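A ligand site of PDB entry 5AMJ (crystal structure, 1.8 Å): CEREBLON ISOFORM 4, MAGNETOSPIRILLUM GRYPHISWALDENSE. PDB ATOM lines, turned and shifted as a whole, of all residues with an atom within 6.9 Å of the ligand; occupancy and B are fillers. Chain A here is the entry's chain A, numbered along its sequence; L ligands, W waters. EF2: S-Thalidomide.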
ATOM      1  N   VAL A  49      -7.760   9.470  36.048  1.00  0.00           N
ATOM      2  CA  VAL A  49      -9.200   9.762  36.056  1.00  0.00           C
ATOM      3  C   VAL A  49     -10.007   8.599  35.505  1.00  0.00           C
ATOM      4  O   VAL A  49      -9.490   7.787  34.772  1.00  0.00           O
ATOM      5  CB  VAL A  49      -9.532  11.013  35.191  1.00  0.00           C
ATOM      6  CG1 VAL A  49      -8.906  12.242  35.863  1.00  0.00           C
ATOM      7  CG2 VAL A  49      -9.030  10.923  33.772  1.00  0.00           C
ATOM      8  N   PHE A  50     -11.285   8.571  35.835  1.00  0.00           N
ATOM      9  CA  PHE A  50     -12.233   7.589  35.327  1.00  0.00           C
ATOM     10  C   PHE A  50     -13.389   8.319  34.630  1.00  0.00           C
ATOM     11  O   PHE A  50     -13.872   9.352  35.106  1.00  0.00           O
ATOM     12  CB  PHE A  50     -12.883   6.765  36.456  1.00  0.00           C
ATOM     13  CG  PHE A  50     -11.953   5.859  37.179  1.00  0.00           C
ATOM     14  CD1 PHE A  50     -11.285   6.305  38.307  1.00  0.00           C
ATOM     15  CD2 PHE A  50     -11.799   4.524  36.798  1.00  0.00           C
ATOM     16  CE1 PHE A  50     -10.436   5.434  39.014  1.00  0.00           C
ATOM     17  CE2 PHE A  50     -10.950   3.653  37.505  1.00  0.00           C
ATOM     18  CZ  PHE A  50     -10.264   4.111  38.606  1.00  0.00           C
ATOM     19  N   ASN A  51     -13.887   7.716  33.554  1.00  0.00           N
ATOM     20  CA  ASN A  51     -15.100   8.177  32.925  1.00  0.00           C
ATOM     21  C   ASN A  51     -16.353   7.474  33.429  1.00  0.00           C
ATOM     22  O   ASN A  51     -16.266   6.564  34.242  1.00  0.00           O
ATOM     23  CB  ASN A  51     -14.906   8.156  31.407  1.00  0.00           C
ATOM     24  CG  ASN A  51     -14.967   6.768  30.803  1.00  0.00           C
ATOM     25  OD1 ASN A  51     -15.288   5.803  31.457  1.00  0.00           O
ATOM     26  ND2 ASN A  51     -14.678   6.704  29.529  1.00  0.00           N
ATOM     27  N   PRO A  52     -17.567   7.922  33.021  1.00  0.00           N
ATOM     28  CA  PRO A  52     -18.792   7.295  33.451  1.00  0.00           C
ATOM     29  C   PRO A  52     -18.960   5.804  33.086  1.00  0.00           C
ATOM     30  O   PRO A  52     -19.814   5.155  33.657  1.00  0.00           O
ATOM     31  CB  PRO A  52     -19.903   8.143  32.790  1.00  0.00           C
ATOM     32  CG  PRO A  52     -19.230   9.428  32.402  1.00  0.00           C
ATOM     33  CD  PRO A  52     -17.828   9.092  32.124  1.00  0.00           C
ATOM     34  N   ALA A  53     -18.199   5.376  32.105  1.00  0.00           N
ATOM     35  CA  ALA A  53     -18.204   3.969  31.663  1.00  0.00           C
ATOM     36  C   ALA A  53     -17.142   3.154  32.445  1.00  0.00           C
ATOM     37  O   ALA A  53     -16.966   1.973  32.159  1.00  0.00           O
ATOM     38  CB  ALA A  53     -17.903   3.893  30.163  1.00  0.00           C
ATOM     39  N   MET A  55     -13.913   3.417  32.728  1.00  0.00           N
ATOM     40  CA  MET A  55     -12.577   3.371  32.149  1.00  0.00           C
ATOM     41  C   MET A  55     -11.631   4.331  32.879  1.00  0.00           C
ATOM     42  O   MET A  55     -11.983   5.501  33.118  1.00  0.00           O
ATOM     43  CB  MET A  55     -12.601   3.679  30.643  1.00  0.00           C
ATOM     44  CG  MET A  55     -13.644   2.816  29.912  1.00  0.00           C
ATOM     45  SD  MET A  55     -13.708   3.308  28.173  1.00  0.00           S
ATOM     46  CE  MET A  55     -15.154   4.334  27.925  1.00  0.00           C
ATOM     47  N   PHE A  57      -8.044   6.327  32.869  1.00  0.00           N
ATOM     48  CA  PHE A  57      -7.079   6.910  31.926  1.00  0.00           C
ATOM     49  C   PHE A  57      -5.989   7.607  32.719  1.00  0.00           C
ATOM     50  O   PHE A  57      -6.262   8.368  33.679  1.00  0.00           O
ATOM     51  CB  PHE A  57      -7.740   7.960  31.037  1.00  0.00           C
ATOM     52  CG  PHE A  57      -8.899   7.453  30.220  1.00  0.00           C
ATOM     53  CD1 PHE A  57      -8.677   6.695  29.067  1.00  0.00           C
ATOM     54  CD2 PHE A  57     -10.194   7.670  30.592  1.00  0.00           C
ATOM     55  CE1 PHE A  57      -9.750   6.201  28.327  1.00  0.00           C
ATOM     56  CE2 PHE A  57     -11.258   7.202  29.817  1.00  0.00           C
ATOM     57  CZ  PHE A  57     -11.022   6.503  28.669  1.00  0.00           C
ATOM     58  N   SER A  75     -18.583  20.288  25.516  1.00  0.00           N
ATOM     59  CA  SER A  75     -19.454  19.971  26.613  1.00  0.00           C
ATOM     60  C   SER A  75     -18.784  20.111  28.000  1.00  0.00           C
ATOM     61  O   SER A  75     -17.640  19.718  28.166  1.00  0.00           O
ATOM     62  CB  SER A  75     -19.923  18.531  26.430  1.00  0.00           C
ATOM     63  OG  SER A  75     -20.724  18.244  27.535  1.00  0.00           O
ATOM     64  N   GLY A  76     -19.523  20.577  29.004  1.00  0.00           N
ATOM     65  CA  GLY A  76     -19.003  20.668  30.368  1.00  0.00           C
ATOM     66  C   GLY A  76     -19.244  19.426  31.213  1.00  0.00           C
ATOM     67  O   GLY A  76     -18.662  19.237  32.299  1.00  0.00           O
ATOM     68  N   GLU A  77     -20.121  18.560  30.721  1.00  0.00           N
ATOM     69  CA  GLU A  77     -20.594  17.404  31.472  1.00  0.00           C
ATOM     70  C   GLU A  77     -19.428  16.491  31.863  1.00  0.00           C
ATOM     71  O   GLU A  77     -18.643  16.132  30.979  1.00  0.00           O
ATOM     72  CB  GLU A  77     -21.578  16.568  30.615  1.00  0.00           C
ATOM     73  CG  GLU A  77     -22.676  17.351  29.898  1.00  0.00           C
ATOM     74  CD  GLU A  77     -23.301  16.595  28.709  1.00  0.00           C
ATOM     75  OE1 GLU A  77     -24.172  15.716  28.943  1.00  0.00           O
ATOM     76  OE2 GLU A  77     -22.909  16.861  27.540  1.00  0.00           O
ATOM     77  N   PHE A  78     -19.360  16.062  33.125  1.00  0.00           N
ATOM     78  CA  PHE A  78     -18.323  15.109  33.613  1.00  0.00           C
ATOM     79  C   PHE A  78     -16.894  15.603  33.413  1.00  0.00           C
ATOM     80  O   PHE A  78     -15.971  14.816  33.493  1.00  0.00           O
ATOM     81  CB  PHE A  78     -18.429  13.721  32.972  1.00  0.00           C
ATOM     82  CG  PHE A  78     -19.817  13.113  32.982  1.00  0.00           C
ATOM     83  CD1 PHE A  78     -20.388  12.682  34.139  1.00  0.00           C
ATOM     84  CD2 PHE A  78     -20.509  12.922  31.792  1.00  0.00           C
ATOM     85  CE1 PHE A  78     -21.687  12.153  34.159  1.00  0.00           C
ATOM     86  CE2 PHE A  78     -21.784  12.382  31.795  1.00  0.00           C
ATOM     87  CZ  PHE A  78     -22.357  11.995  32.962  1.00  0.00           C
ATOM     88  N   SER A  79     -16.681  16.882  33.094  1.00  0.00           N
ATOM     89  CA  SER A  79     -15.337  17.380  32.869  1.00  0.00           C
ATOM     90  C   SER A  79     -14.478  17.105  34.087  1.00  0.00           C
ATOM     91  O   SER A  79     -14.889  17.432  35.196  1.00  0.00           O
ATOM     92  CB  SER A  79     -15.348  18.919  32.661  1.00  0.00           C
ATOM     93  OG  SER A  79     -14.007  19.305  32.387  1.00  0.00           O
ATOM     94  N   TRP A  80     -13.286  16.571  33.872  1.00  0.00           N
ATOM     95  CA  TRP A  80     -12.346  16.375  34.934  1.00  0.00           C
ATOM     96  C   TRP A  80     -11.603  17.628  35.356  1.00  0.00           C
ATOM     97  O   TRP A  80     -10.937  17.639  36.400  1.00  0.00           O
ATOM     98  CB  TRP A  80     -11.316  15.348  34.520  1.00  0.00           C
ATOM     99  CG  TRP A  80     -11.906  13.977  34.228  1.00  0.00           C
ATOM    100  CD1 TRP A  80     -12.701  13.201  35.025  1.00  0.00           C
ATOM    101  CD2 TRP A  80     -11.668  13.233  33.070  1.00  0.00           C
ATOM    102  NE1 TRP A  80     -12.973  12.017  34.392  1.00  0.00           N
ATOM    103  CE2 TRP A  80     -12.362  12.004  33.189  1.00  0.00           C
ATOM    104  CE3 TRP A  80     -10.929  13.482  31.923  1.00  0.00           C
ATOM    105  CZ2 TRP A  80     -12.328  11.035  32.218  1.00  0.00           C
ATOM    106  CZ3 TRP A  80     -10.864  12.534  30.953  1.00  0.00           C
ATOM    107  CH2 TRP A  80     -11.593  11.319  31.084  1.00  0.00           C
ATOM    108  N   PHE A  81     -11.764  18.721  34.617  1.00  0.00           N
ATOM    109  CA  PHE A  81     -11.049  19.977  34.911  1.00  0.00           C
ATOM    110  C   PHE A  81     -12.064  21.097  35.024  1.00  0.00           C
ATOM    111  O   PHE A  81     -12.762  21.418  34.079  1.00  0.00           O
ATOM    112  CB  PHE A  81     -10.070  20.235  33.802  1.00  0.00           C
ATOM    113  CG  PHE A  81      -9.078  19.123  33.612  1.00  0.00           C
ATOM    114  CD1 PHE A  81      -7.913  19.059  34.387  1.00  0.00           C
ATOM    115  CD2 PHE A  81      -9.254  18.169  32.627  1.00  0.00           C
ATOM    116  CE1 PHE A  81      -6.995  18.023  34.189  1.00  0.00           C
ATOM    117  CE2 PHE A  81      -8.308  17.146  32.430  1.00  0.00           C
ATOM    118  CZ  PHE A  81      -7.195  17.080  33.222  1.00  0.00           C
ATOM    119  N   TYR A  84     -13.680  23.987  32.452  1.00  0.00           N
ATOM    120  CA  TYR A  84     -13.445  23.667  31.032  1.00  0.00           C
ATOM    121  C   TYR A  84     -14.526  22.788  30.409  1.00  0.00           C
ATOM    122  O   TYR A  84     -15.080  21.907  31.106  1.00  0.00           O
ATOM    123  CB  TYR A  84     -12.068  22.979  30.844  1.00  0.00           C
ATOM    124  CG  TYR A  84     -10.906  23.803  31.263  1.00  0.00           C
ATOM    125  CD1 TYR A  84     -10.440  23.745  32.564  1.00  0.00           C
ATOM    126  CD2 TYR A  84     -10.238  24.638  30.349  1.00  0.00           C
ATOM    127  CE1 TYR A  84      -9.342  24.536  32.962  1.00  0.00           C
ATOM    128  CE2 TYR A  84      -9.154  25.374  30.701  1.00  0.00           C
ATOM    129  CZ  TYR A  84      -8.705  25.349  32.049  1.00  0.00           C
ATOM    130  OH  TYR A  84      -7.676  26.126  32.492  1.00  0.00           O
ATOM    131  N   TRP A  86     -15.160  20.133  27.061  1.00  0.00           N
ATOM    132  CA  TRP A  86     -14.295  19.269  26.256  1.00  0.00           C
ATOM    133  C   TRP A  86     -14.892  18.879  24.934  1.00  0.00           C
ATOM    134  O   TRP A  86     -16.098  18.846  24.766  1.00  0.00           O
ATOM    135  CB  TRP A  86     -13.947  17.968  27.022  1.00  0.00           C
ATOM    136  CG  TRP A  86     -15.151  17.242  27.563  1.00  0.00           C
ATOM    137  CD1 TRP A  86     -15.738  17.433  28.807  1.00  0.00           C
ATOM    138  CD2 TRP A  86     -15.954  16.284  26.891  1.00  0.00           C
ATOM    139  NE1 TRP A  86     -16.798  16.656  28.923  1.00  0.00           N
ATOM    140  CE2 TRP A  86     -16.998  15.923  27.782  1.00  0.00           C
ATOM    141  CE3 TRP A  86     -15.912  15.705  25.593  1.00  0.00           C
ATOM    142  CZ2 TRP A  86     -17.982  14.987  27.454  1.00  0.00           C
ATOM    143  CZ3 TRP A  86     -16.899  14.741  25.288  1.00  0.00           C
ATOM    144  CH2 TRP A  86     -17.930  14.412  26.216  1.00  0.00           C
ATOM    145  N   THR A  87     -14.020  18.596  23.956  1.00  0.00           N
ATOM    146  CA  THR A  87     -14.363  17.983  22.713  1.00  0.00           C
ATOM    147  C   THR A  87     -13.469  16.755  22.527  1.00  0.00           C
ATOM    148  O   THR A  87     -12.350  16.703  23.042  1.00  0.00           O
ATOM    149  CB  THR A  87     -14.192  18.926  21.519  1.00  0.00           C
ATOM    150  OG1 THR A  87     -12.830  19.320  21.438  1.00  0.00           O
ATOM    151  CG2 THR A  87     -15.012  20.113  21.670  1.00  0.00           C
ATOM    152  N   ILE A  88     -13.971  15.748  21.840  1.00  0.00           N
ATOM    153  CA  ILE A  88     -13.177  14.578  21.518  1.00  0.00           C
ATOM    154  C   ILE A  88     -12.027  14.914  20.539  1.00  0.00           C
ATOM    155  O   ILE A  88     -12.255  15.589  19.525  1.00  0.00           O
ATOM    156  CB  ILE A  88     -14.106  13.463  21.017  1.00  0.00           C
ATOM    157  CG1 ILE A  88     -14.985  12.990  22.204  1.00  0.00           C
ATOM    158  CG2 ILE A  88     -13.377  12.305  20.379  1.00  0.00           C
ATOM    159  CD1 ILE A  88     -16.218  12.219  21.776  1.00  0.00           C
ATOM    160  N   HIS A  97      -8.891   7.277  19.126  1.00  0.00           N
ATOM    161  CA  HIS A  97      -9.251   8.262  20.109  1.00  0.00           C
ATOM    162  C   HIS A  97      -8.043   8.515  21.062  1.00  0.00           C
ATOM    163  O   HIS A  97      -7.704   7.684  21.906  1.00  0.00           O
ATOM    164  CB  HIS A  97     -10.527   7.821  20.858  1.00  0.00           C
ATOM    165  CG  HIS A  97     -10.883   8.777  21.956  1.00  0.00           C
ATOM    166  ND1 HIS A  97     -11.504   8.384  23.119  1.00  0.00           N
ATOM    167  CD2 HIS A  97     -10.675  10.105  22.080  1.00  0.00           C
ATOM    168  CE1 HIS A  97     -11.714   9.439  23.893  1.00  0.00           C
ATOM    169  NE2 HIS A  97     -11.162  10.484  23.308  1.00  0.00           N
ATOM    170  N   TRP A 100      -8.789  14.438  24.576  1.00  0.00           N
ATOM    171  CA  TRP A 100      -9.801  15.517  24.540  1.00  0.00           C
ATOM    172  C   TRP A 100      -9.129  16.883  24.436  1.00  0.00           C
ATOM    173  O   TRP A 100      -7.994  17.108  24.919  1.00  0.00           O
ATOM    174  CB  TRP A 100     -10.686  15.469  25.794  1.00  0.00           C
ATOM    175  CG  TRP A 100     -11.362  14.169  25.983  1.00  0.00           C
ATOM    176  CD1 TRP A 100     -12.557  13.805  25.512  1.00  0.00           C
ATOM    177  CD2 TRP A 100     -10.826  13.036  26.651  1.00  0.00           C
ATOM    178  NE1 TRP A 100     -12.820  12.506  25.870  1.00  0.00           N
ATOM    179  CE2 TRP A 100     -11.775  12.014  26.566  1.00  0.00           C
ATOM    180  CE3 TRP A 100      -9.618  12.794  27.320  1.00  0.00           C
ATOM    181  CZ2 TRP A 100     -11.575  10.754  27.106  1.00  0.00           C
ATOM    182  CZ3 TRP A 100      -9.393  11.501  27.832  1.00  0.00           C
ATOM    183  CH2 TRP A 100     -10.367  10.517  27.733  1.00  0.00           C
ATOM    184  N   TYR A 102      -9.676  20.763  25.704  1.00  0.00           N
ATOM    185  CA  TYR A 102     -10.410  21.545  26.700  1.00  0.00           C
ATOM    186  C   TYR A 102     -10.355  22.999  26.345  1.00  0.00           C
ATOM    187  O   TYR A 102      -9.299  23.534  25.910  1.00  0.00           O
ATOM    188  CB  TYR A 102      -9.762  21.299  28.092  1.00  0.00           C
ATOM    189  CG  TYR A 102     -10.016  19.905  28.554  1.00  0.00           C
ATOM    190  CD1 TYR A 102     -11.210  19.597  29.230  1.00  0.00           C
ATOM    191  CD2 TYR A 102      -9.147  18.855  28.288  1.00  0.00           C
ATOM    192  CE1 TYR A 102     -11.466  18.287  29.691  1.00  0.00           C
ATOM    193  CE2 TYR A 102      -9.413  17.573  28.688  1.00  0.00           C
ATOM    194  CZ  TYR A 102     -10.578  17.272  29.408  1.00  0.00           C
ATOM    195  OH  TYR A 102     -10.859  15.975  29.813  1.00  0.00           O
HETATM  196  O01 EF2 L   1     -15.661  11.675  31.592  1.00  0.00           O
HETATM  197  C02 EF2 L   1     -15.068  12.418  30.832  1.00  0.00           C
HETATM  198  N03 EF2 L   1     -14.535  13.634  31.335  1.00  0.00           N
HETATM  199  C04 EF2 L   1     -13.786  14.550  30.509  1.00  0.00           C
HETATM  200  O05 EF2 L   1     -13.287  15.523  31.018  1.00  0.00           O
HETATM  201  C06 EF2 L   1     -13.646  14.196  29.079  1.00  0.00           C
HETATM  202  C07 EF2 L   1     -14.773  13.355  28.543  1.00  0.00           C
HETATM  203  C08 EF2 L   1     -14.885  12.097  29.355  1.00  0.00           C
HETATM  204  N09 EF2 L   1     -15.953  11.236  29.064  1.00  0.00           N
HETATM  205  C11 EF2 L   1     -19.015   7.851  27.865  1.00  0.00           C
HETATM  206  C12 EF2 L   1     -17.640   8.061  27.868  1.00  0.00           C
HETATM  207  C13 EF2 L   1     -17.193   9.335  28.346  1.00  0.00           C
HETATM  208  C14 EF2 L   1     -18.068  10.296  28.732  1.00  0.00           C
HETATM  209  O16 EF2 L   1     -14.631   9.415  28.370  1.00  0.00           O
HETATM  210  O18 EF2 L   1     -17.770  12.648  29.668  1.00  0.00           O
HETATM  211  C19 EF2 L   1     -19.438  10.115  28.715  1.00  0.00           C
HETATM  212  C20 EF2 L   1     -19.872   8.846  28.233  1.00  0.00           C
HETATM  213  C3  EF2 L   1     -17.356  11.528  29.080  1.00  0.00           C
HETATM  214  C4  EF2 L   1     -15.882   9.922  28.468  1.00  0.00           C
HETATM  215  O   HOH W   1     -15.258  10.841  25.354  1.00  0.00           O
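The side-chain amide oxygen (OD1) of Asn 51 lies within hydrogen-bond range of the backbone NH (N) of Met 55, at 3.0 Å. The side-chain amide oxygen (OD1) of Asn 51 lies within hydrogen-bond range of the backbone NH (N) of Ala 53. NE1 of Trp 80 is in hydrogen-bond range of O of Phe 50 (2.9 Å). The backbone carbonyl oxygen of Glu 77 sits at hydrogen-bond distance from the indole nitrogen of Trp 86 (2.8 Å). N of Trp 86 sits at hydrogen-bond distance from O of Ser 75 (2.7 Å). The side-chain hydroxyl (OG) of Ser 79 sits at hydrogen-bond distance from the backbone carbonyl oxygen (O) of Phe 81 (3.0 Å). The backbone carbonyl oxygen (O) of Tyr 84 lies within hydrogen-bond range of the side-chain hydroxyl (OG) of Ser 79 (3.1 Å). The side-chain carboxylate of Glu 77 lies within hydrogen-bond range of the side-chain hydroxyl of Ser 75, 2.6 Å away.
Water W1 bridges NE1 of Trp 100 and O16 of the ligand.
The side-chain hydroxyl (OH) of Tyr 102 lies within hydrogen-bond range of an oxygen (O05) of the ligand (2.7 Å). O of Phe 78 is in hydrogen-bond range of N03 of the ligand, 2.8 Å away. ND2 of Asn 51 lies within hydrogen-bond range of O16 of the ligand. The backbone NH of Trp 80 is in hydrogen-bond range of an oxygen (O05) of the ligand.
Pro 52 touches the ligand. Glu 77 touches the ligand. Ser 79 touches the ligand (CA to O05, 3.3 Å). Trp 86 touches the ligand (CZ2 to O18, 3.2 Å). Trp 100 touches the ligand (NE1 to C07, 3.4 Å). Nine residues have an atom within 4 Å of the ligand: Asn 51, Pro 52, Glu 77, Phe 78, Ser 79, Trp 80, Trp 86, Trp 100 and Tyr 102. The nearest printed residue that does not touch the ligand is Phe 57 (4.3 Å).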
